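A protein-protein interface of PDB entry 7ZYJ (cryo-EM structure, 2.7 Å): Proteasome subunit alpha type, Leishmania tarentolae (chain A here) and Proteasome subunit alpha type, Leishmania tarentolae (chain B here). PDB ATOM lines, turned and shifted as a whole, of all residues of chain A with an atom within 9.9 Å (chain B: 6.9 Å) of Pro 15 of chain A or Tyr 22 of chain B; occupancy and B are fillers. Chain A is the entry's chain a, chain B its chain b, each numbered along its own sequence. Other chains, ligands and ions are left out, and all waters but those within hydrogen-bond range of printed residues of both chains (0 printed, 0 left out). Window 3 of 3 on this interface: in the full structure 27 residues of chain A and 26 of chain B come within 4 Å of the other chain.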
ATOM      1  N   ALA A   4     -12.856  11.425  31.724  1.00  0.00           N
ATOM      2  CA  ALA A   4     -12.018  12.611  31.598  1.00  0.00           C
ATOM      3  C   ALA A   4     -10.692  12.421  32.324  1.00  0.00           C
ATOM      4  O   ALA A   4      -9.858  13.327  32.363  1.00  0.00           O
ATOM      5  CB  ALA A   4     -12.747  13.836  32.133  1.00  0.00           C
ATOM      6  N   GLY A   5     -10.504  11.238  32.900  1.00  0.00           N
ATOM      7  CA  GLY A   5      -9.297  10.948  33.647  1.00  0.00           C
ATOM      8  C   GLY A   5      -8.225  10.253  32.834  1.00  0.00           C
ATOM      9  O   GLY A   5      -7.039  10.566  32.966  1.00  0.00           O
ATOM     10  N   PHE A   6      -8.627   9.303  31.988  1.00  0.00           N
ATOM     11  CA  PHE A   6      -7.650   8.503  31.251  1.00  0.00           C
ATOM     12  C   PHE A   6      -7.137   9.240  30.015  1.00  0.00           C
ATOM     13  O   PHE A   6      -5.938   9.493  29.889  1.00  0.00           O
ATOM     14  CB  PHE A   6      -8.260   7.145  30.875  1.00  0.00           C
ATOM     15  CG  PHE A   6      -9.710   7.212  30.457  1.00  0.00           C
ATOM     16  CD1 PHE A   6     -10.724   7.174  31.403  1.00  0.00           C
ATOM     17  CD2 PHE A   6     -10.058   7.291  29.117  1.00  0.00           C
ATOM     18  CE1 PHE A   6     -12.052   7.233  31.022  1.00  0.00           C
ATOM     19  CE2 PHE A   6     -11.385   7.351  28.731  1.00  0.00           C
ATOM     20  CZ  PHE A   6     -12.382   7.321  29.685  1.00  0.00           C
ATOM     21  N   ASP A   7      -8.035   9.516  29.065  1.00  0.00           N
ATOM     22  CA  ASP A   7      -7.862  10.336  27.861  1.00  0.00           C
ATOM     23  C   ASP A   7      -6.656   9.911  27.024  1.00  0.00           C
ATOM     24  O   ASP A   7      -6.283  10.607  26.075  1.00  0.00           O
ATOM     25  CB  ASP A   7      -7.820  11.845  28.199  1.00  0.00           C
ATOM     26  CG  ASP A   7      -6.465  12.356  28.716  1.00  0.00           C
ATOM     27  OD1 ASP A   7      -5.455  11.633  28.776  1.00  0.00           O
ATOM     28  OD2 ASP A   7      -6.420  13.551  29.077  1.00  0.00           O
ATOM     29  N   LYS A   8      -6.044   8.772  27.360  1.00  0.00           N
ATOM     30  CA  LYS A   8      -4.853   8.326  26.648  1.00  0.00           C
ATOM     31  C   LYS A   8      -4.822   6.819  26.419  1.00  0.00           C
ATOM     32  O   LYS A   8      -3.830   6.313  25.880  1.00  0.00           O
ATOM     33  CB  LYS A   8      -3.587   8.758  27.399  1.00  0.00           C
ATOM     34  CG  LYS A   8      -3.342   8.016  28.699  1.00  0.00           C
ATOM     35  CD  LYS A   8      -2.096   8.539  29.394  1.00  0.00           C
ATOM     36  CE  LYS A   8      -2.089  10.059  29.441  1.00  0.00           C
ATOM     37  NZ  LYS A   8      -0.847  10.590  30.063  1.00  0.00           N
ATOM     38  N   VAL A  12      -9.117   9.235  21.800  1.00  0.00           N
ATOM     39  CA  VAL A  12      -9.839  10.462  22.108  1.00  0.00           C
ATOM     40  C   VAL A  12      -8.823  11.585  22.244  1.00  0.00           C
ATOM     41  O   VAL A  12      -7.653  11.353  22.564  1.00  0.00           O
ATOM     42  CB  VAL A  12     -10.692  10.336  23.390  1.00  0.00           C
ATOM     43  CG1 VAL A  12     -11.857   9.387  23.163  1.00  0.00           C
ATOM     44  CG2 VAL A  12      -9.836   9.871  24.556  1.00  0.00           C
ATOM     45  N   PHE A  13      -9.275  12.809  21.992  1.00  0.00           N
ATOM     46  CA  PHE A  13      -8.377  13.953  22.047  1.00  0.00           C
ATOM     47  C   PHE A  13      -7.969  14.266  23.479  1.00  0.00           C
ATOM     48  O   PHE A  13      -8.782  14.200  24.408  1.00  0.00           O
ATOM     49  CB  PHE A  13      -9.032  15.181  21.421  1.00  0.00           C
ATOM     50  CG  PHE A  13      -9.130  15.120  19.928  1.00  0.00           C
ATOM     51  CD1 PHE A  13      -8.052  15.473  19.136  1.00  0.00           C
ATOM     52  CD2 PHE A  13     -10.302  14.719  19.315  1.00  0.00           C
ATOM     53  CE1 PHE A  13      -8.140  15.420  17.761  1.00  0.00           C
ATOM     54  CE2 PHE A  13     -10.394  14.665  17.943  1.00  0.00           C
ATOM     55  CZ  PHE A  13      -9.313  15.016  17.164  1.00  0.00           C
ATOM     56  N   SER A  14      -6.699  14.603  23.652  1.00  0.00           N
ATOM     57  CA  SER A  14      -6.200  15.161  24.896  1.00  0.00           C
ATOM     58  C   SER A  14      -6.595  16.628  24.982  1.00  0.00           C
ATOM     59  O   SER A  14      -7.015  17.230  23.992  1.00  0.00           O
ATOM     60  CB  SER A  14      -4.684  14.985  24.965  1.00  0.00           C
ATOM     61  OG  SER A  14      -4.035  15.772  23.982  1.00  0.00           O
ATOM     62  N   PRO A  15      -6.492  17.240  26.165  1.00  0.00           N
ATOM     63  CA  PRO A  15      -6.774  18.681  26.263  1.00  0.00           C
ATOM     64  C   PRO A  15      -5.880  19.535  25.382  1.00  0.00           C
ATOM     65  O   PRO A  15      -6.250  20.672  25.066  1.00  0.00           O
ATOM     66  CB  PRO A  15      -6.549  18.982  27.750  1.00  0.00           C
ATOM     67  CG  PRO A  15      -6.814  17.688  28.429  1.00  0.00           C
ATOM     68  CD  PRO A  15      -6.308  16.629  27.494  1.00  0.00           C
ATOM     69  N   GLU A  16      -4.721  19.025  24.973  1.00  0.00           N
ATOM     70  CA  GLU A  16      -3.820  19.730  24.074  1.00  0.00           C
ATOM     71  C   GLU A  16      -4.122  19.457  22.606  1.00  0.00           C
ATOM     72  O   GLU A  16      -3.381  19.931  21.738  1.00  0.00           O
ATOM     73  CB  GLU A  16      -2.364  19.353  24.375  1.00  0.00           C
ATOM     74  CG  GLU A  16      -1.831  19.865  25.708  1.00  0.00           C
ATOM     75  CD  GLU A  16      -2.459  19.175  26.904  1.00  0.00           C
ATOM     76  OE1 GLU A  16      -2.197  17.971  27.104  1.00  0.00           O
ATOM     77  OE2 GLU A  16      -3.216  19.838  27.644  1.00  0.00           O
ATOM     78  N   GLY A  17      -5.180  18.710  22.309  1.00  0.00           N
ATOM     79  CA  GLY A  17      -5.511  18.392  20.934  1.00  0.00           C
ATOM     80  C   GLY A  17      -4.595  17.379  20.289  1.00  0.00           C
ATOM     81  O   GLY A  17      -4.265  17.511  19.103  1.00  0.00           O
ATOM     82  N   SER A  18      -4.168  16.365  21.037  1.00  0.00           N
ATOM     83  CA  SER A  18      -3.282  15.334  20.525  1.00  0.00           C
ATOM     84  C   SER A  18      -3.851  13.962  20.856  1.00  0.00           C
ATOM     85  O   SER A  18      -4.643  13.802  21.787  1.00  0.00           O
ATOM     86  CB  SER A  18      -1.866  15.471  21.101  1.00  0.00           C
ATOM     87  OG  SER A  18      -1.854  15.198  22.490  1.00  0.00           O
ATOM     88  N   LEU A  19      -3.436  12.969  20.076  1.00  0.00           N
ATOM     89  CA  LEU A  19      -3.851  11.584  20.262  1.00  0.00           C
ATOM     90  C   LEU A  19      -2.684  10.822  20.875  1.00  0.00           C
ATOM     91  O   LEU A  19      -1.673  10.581  20.208  1.00  0.00           O
ATOM     92  CB  LEU A  19      -4.286  10.963  18.937  1.00  0.00           C
ATOM     93  CG  LEU A  19      -5.437  11.657  18.208  1.00  0.00           C
ATOM     94  CD1 LEU A  19      -5.524  11.173  16.771  1.00  0.00           C
ATOM     95  CD2 LEU A  19      -6.749  11.423  18.937  1.00  0.00           C
ATOM     96  N   TYR A  20      -2.826  10.448  22.149  1.00  0.00           N
ATOM     97  CA  TYR A  20      -1.730   9.794  22.855  1.00  0.00           C
ATOM     98  C   TYR A  20      -1.481   8.388  22.324  1.00  0.00           C
ATOM     99  O   TYR A  20      -0.328   7.952  22.228  1.00  0.00           O
ATOM    100  CB  TYR A  20      -2.024   9.756  24.353  1.00  0.00           C
ATOM    101  CG  TYR A  20      -1.565  10.991  25.092  1.00  0.00           C
ATOM    102  CD1 TYR A  20      -0.219  11.311  25.179  1.00  0.00           C
ATOM    103  CD2 TYR A  20      -2.482  11.838  25.700  1.00  0.00           C
ATOM    104  CE1 TYR A  20       0.204  12.439  25.854  1.00  0.00           C
ATOM    105  CE2 TYR A  20      -2.069  12.968  26.377  1.00  0.00           C
ATOM    106  CZ  TYR A  20      -0.724  13.264  26.450  1.00  0.00           C
ATOM    107  OH  TYR A  20      -0.308  14.390  27.123  1.00  0.00           O
ATOM    108  N   LEU B  17     -19.324  20.432  25.198  1.00  0.00           N
ATOM    109  CA  LEU B  17     -18.862  19.166  24.632  1.00  0.00           C
ATOM    110  C   LEU B  17     -17.346  19.264  24.525  1.00  0.00           C
ATOM    111  O   LEU B  17     -16.798  19.679  23.503  1.00  0.00           O
ATOM    112  CB  LEU B  17     -19.526  18.899  23.288  1.00  0.00           C
ATOM    113  CG  LEU B  17     -21.053  18.799  23.337  1.00  0.00           C
ATOM    114  CD1 LEU B  17     -21.670  19.070  21.977  1.00  0.00           C
ATOM    115  CD2 LEU B  17     -21.472  17.435  23.851  1.00  0.00           C
ATOM    116  N   ILE B  18     -16.662  18.881  25.607  1.00  0.00           N
ATOM    117  CA  ILE B  18     -15.228  19.132  25.718  1.00  0.00           C
ATOM    118  C   ILE B  18     -14.446  18.368  24.658  1.00  0.00           C
ATOM    119  O   ILE B  18     -13.358  18.797  24.259  1.00  0.00           O
ATOM    120  CB  ILE B  18     -14.736  18.794  27.138  1.00  0.00           C
ATOM    121  CG1 ILE B  18     -14.827  17.291  27.400  1.00  0.00           C
ATOM    122  CG2 ILE B  18     -15.534  19.565  28.175  1.00  0.00           C
ATOM    123  CD1 ILE B  18     -14.177  16.859  28.693  1.00  0.00           C
ATOM    124  N   GLN B  19     -14.967  17.234  24.189  1.00  0.00           N
ATOM    125  CA  GLN B  19     -14.293  16.515  23.116  1.00  0.00           C
ATOM    126  C   GLN B  19     -14.281  17.326  21.827  1.00  0.00           C
ATOM    127  O   GLN B  19     -13.266  17.355  21.120  1.00  0.00           O
ATOM    128  CB  GLN B  19     -14.963  15.158  22.894  1.00  0.00           C
ATOM    129  CG  GLN B  19     -14.032  14.102  22.337  1.00  0.00           C
ATOM    130  CD  GLN B  19     -12.884  13.795  23.275  1.00  0.00           C
ATOM    131  OE1 GLN B  19     -11.746  14.194  23.033  1.00  0.00           O
ATOM    132  NE2 GLN B  19     -13.177  13.084  24.356  1.00  0.00           N
ATOM    133  N   ILE B  20     -15.386  18.006  21.516  1.00  0.00           N
ATOM    134  CA  ILE B  20     -15.428  18.858  20.332  1.00  0.00           C
ATOM    135  C   ILE B  20     -14.496  20.052  20.497  1.00  0.00           C
ATOM    136  O   ILE B  20     -13.849  20.486  19.538  1.00  0.00           O
ATOM    137  CB  ILE B  20     -16.875  19.296  20.044  1.00  0.00           C
ATOM    138  CG1 ILE B  20     -17.763  18.071  19.822  1.00  0.00           C
ATOM    139  CG2 ILE B  20     -16.926  20.216  18.840  1.00  0.00           C
ATOM    140  CD1 ILE B  20     -19.183  18.410  19.440  1.00  0.00           C
ATOM    141  N   GLU B  21     -14.411  20.604  21.709  1.00  0.00           N
ATOM    142  CA  GLU B  21     -13.482  21.704  21.953  1.00  0.00           C
ATOM    143  C   GLU B  21     -12.037  21.255  21.776  1.00  0.00           C
ATOM    144  O   GLU B  21     -11.217  21.985  21.206  1.00  0.00           O
ATOM    145  CB  GLU B  21     -13.705  22.276  23.353  1.00  0.00           C
ATOM    146  CG  GLU B  21     -12.716  23.359  23.750  1.00  0.00           C
ATOM    147  CD  GLU B  21     -12.408  23.350  25.234  1.00  0.00           C
ATOM    148  OE1 GLU B  21     -11.294  23.766  25.615  1.00  0.00           O
ATOM    149  OE2 GLU B  21     -13.280  22.925  26.021  1.00  0.00           O
ATOM    150  N   TYR B  22     -11.705  20.055  22.257  1.00  0.00           N
ATOM    151  CA  TYR B  22     -10.359  19.524  22.066  1.00  0.00           C
ATOM    152  C   TYR B  22     -10.069  19.274  20.592  1.00  0.00           C
ATOM    153  O   TYR B  22      -8.953  19.520  20.121  1.00  0.00           O
ATOM    154  CB  TYR B  22     -10.182  18.241  22.876  1.00  0.00           C
ATOM    155  CG  TYR B  22     -10.234  18.435  24.375  1.00  0.00           C
ATOM    156  CD1 TYR B  22     -10.152  19.703  24.936  1.00  0.00           C
ATOM    157  CD2 TYR B  22     -10.368  17.350  25.229  1.00  0.00           C
ATOM    158  CE1 TYR B  22     -10.202  19.883  26.303  1.00  0.00           C
ATOM    159  CE2 TYR B  22     -10.418  17.520  26.597  1.00  0.00           C
ATOM    160  CZ  TYR B  22     -10.334  18.787  27.128  1.00  0.00           C
ATOM    161  OH  TYR B  22     -10.383  18.963  28.491  1.00  0.00           O
ATOM    162  N   ALA B  23     -11.062  18.778  19.849  1.00  0.00           N
ATOM    163  CA  ALA B  23     -10.890  18.600  18.411  1.00  0.00           C
ATOM    164  C   ALA B  23     -10.673  19.932  17.706  1.00  0.00           C
ATOM    165  O   ALA B  23      -9.875  20.014  16.766  1.00  0.00           O
ATOM    166  CB  ALA B  23     -12.101  17.876  17.823  1.00  0.00           C
ATOM    167  N   THR B  24     -11.383  20.978  18.134  1.00  0.00           N
ATOM    168  CA  THR B  24     -11.163  22.310  17.580  1.00  0.00           C
ATOM    169  C   THR B  24      -9.761  22.811  17.900  1.00  0.00           C
ATOM    170  O   THR B  24      -9.116  23.451  17.062  1.00  0.00           O
ATOM    171  CB  THR B  24     -12.214  23.282  18.117  1.00  0.00           C
ATOM    172  OG1 THR B  24     -13.521  22.723  17.933  1.00  0.00           O
ATOM    173  CG2 THR B  24     -12.132  24.614  17.389  1.00  0.00           C
ATOM    174  N   THR B  25      -9.279  22.534  19.113  1.00  0.00           N
ATOM    175  CA  THR B  25      -7.908  22.889  19.468  1.00  0.00           C
ATOM    176  C   THR B  25      -6.909  22.165  18.574  1.00  0.00           C
ATOM    177  O   THR B  25      -5.906  22.749  18.146  1.00  0.00           O
ATOM    178  CB  THR B  25      -7.643  22.567  20.938  1.00  0.00           C
ATOM    179  OG1 THR B  25      -8.612  23.231  21.757  1.00  0.00           O
ATOM    180  CG2 THR B  25      -6.249  23.021  21.343  1.00  0.00           C
ATOM    181  N   ALA B  26      -7.166  20.887  18.285  1.00  0.00           N
ATOM    182  CA  ALA B  26      -6.312  20.145  17.365  1.00  0.00           C
ATOM    183  C   ALA B  26      -6.369  20.721  15.956  1.00  0.00           C
ATOM    184  O   ALA B  26      -5.354  20.726  15.250  1.00  0.00           O
ATOM    185  CB  ALA B  26      -6.714  18.672  17.347  1.00  0.00           C
ATOM    186  N   ALA B  27      -7.534  21.206  15.532  1.00  0.00           N
ATOM    187  CA  ALA B  27      -7.702  21.764  14.198  1.00  0.00           C
ATOM    188  C   ALA B  27      -6.995  23.100  14.016  1.00  0.00           C
ATOM    189  O   ALA B  27      -6.762  23.508  12.874  1.00  0.00           O
ATOM    190  CB  ALA B  27      -9.191  21.926  13.880  1.00  0.00           C
ATOM    191  N   PHE B 128     -13.504  14.993  14.170  1.00  0.00           N
ATOM    192  CA  PHE B 128     -12.378  15.280  13.297  1.00  0.00           C
ATOM    193  C   PHE B 128     -11.522  16.398  13.881  1.00  0.00           C
ATOM    194  O   PHE B 128     -12.008  17.273  14.600  1.00  0.00           O
ATOM    195  CB  PHE B 128     -12.866  15.670  11.902  1.00  0.00           C
ATOM    196  CG  PHE B 128     -13.514  14.546  11.152  1.00  0.00           C
ATOM    197  CD1 PHE B 128     -12.746  13.581  10.523  1.00  0.00           C
ATOM    198  CD2 PHE B 128     -14.892  14.452  11.075  1.00  0.00           C
ATOM    199  CE1 PHE B 128     -13.340  12.546   9.831  1.00  0.00           C
ATOM    200  CE2 PHE B 128     -15.494  13.419  10.385  1.00  0.00           C
ATOM    201  CZ  PHE B 128     -14.717  12.465   9.762  1.00  0.00           C
ATOM    202  N   GLY B 129     -10.231  16.361  13.563  1.00  0.00           N
ATOM    203  CA  GLY B 129      -9.309  17.358  14.068  1.00  0.00           C
ATOM    204  C   GLY B 129      -8.799  18.299  12.998  1.00  0.00           C
ATOM    205  O   GLY B 129      -7.618  18.654  12.988  1.00  0.00           O
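Of the printed residues of chain B, Gly 17 of chain A touches Tyr 22 and Ala 26. No residue of chain A comes within 4 Å of Glu 21 of chain B. Tyr 22 of chain B touches four residues of chain A. Of chain A, only Phe 13 comes within 4 Å of Ala 23 of chain B. Printed residues of chain A within 4 Å of Ala 26 of chain B: Phe 13 and Gly 17. The nearest printed residue of chain B that does not touch Gly 17 of chain A is Thr 25 of chain B (4.5 Å).
Printed residues of chain A that touch a printed residue of chain B: Val 12, Phe 13, Ser 14, Pro 15 and Gly 17. Hydrophobic or aromatic side chains of chain A within 4 Å of the printed part of chain B: Val 12, Phe 13 and Pro 15.
OG of Ser 14 of chain A is in hydrogen-bond range of OG of Ser 18 of chain A, 2.7 Å away. The backbone NH of Glu 16 of chain A lies close to the side-chain hydroxyl of Ser 14 of chain A.
Among the printed residues, merely in contact across the chains: Gly 17 of chain A with Ala 26 of chain B (3.2 Å), Ser 14 of chain A with Tyr 22 of chain B (3.5 Å), Phe 13 of chain A with Ala 26 of chain B (3.6 Å), Phe 13 of chain A with Tyr 22 of chain B (3.6 Å), Pro 15 of chain A with Tyr 22 of chain B (3.6 Å), Phe 13 of chain A with Ala 23 of chain B (3.6 Å), Gly 17 of chain A with Tyr 22 of chain B (3.7 Å), Val 12 of chain A with Gln 19 of chain B (3.8 Å) and Phe 13 of chain A with Gly 129 of chain B (3.9 Å).
N of Phe 13 of chain A lies within hydrogen-bond range of OE1 of Gln 19 of chain B, at 3.0 Å.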
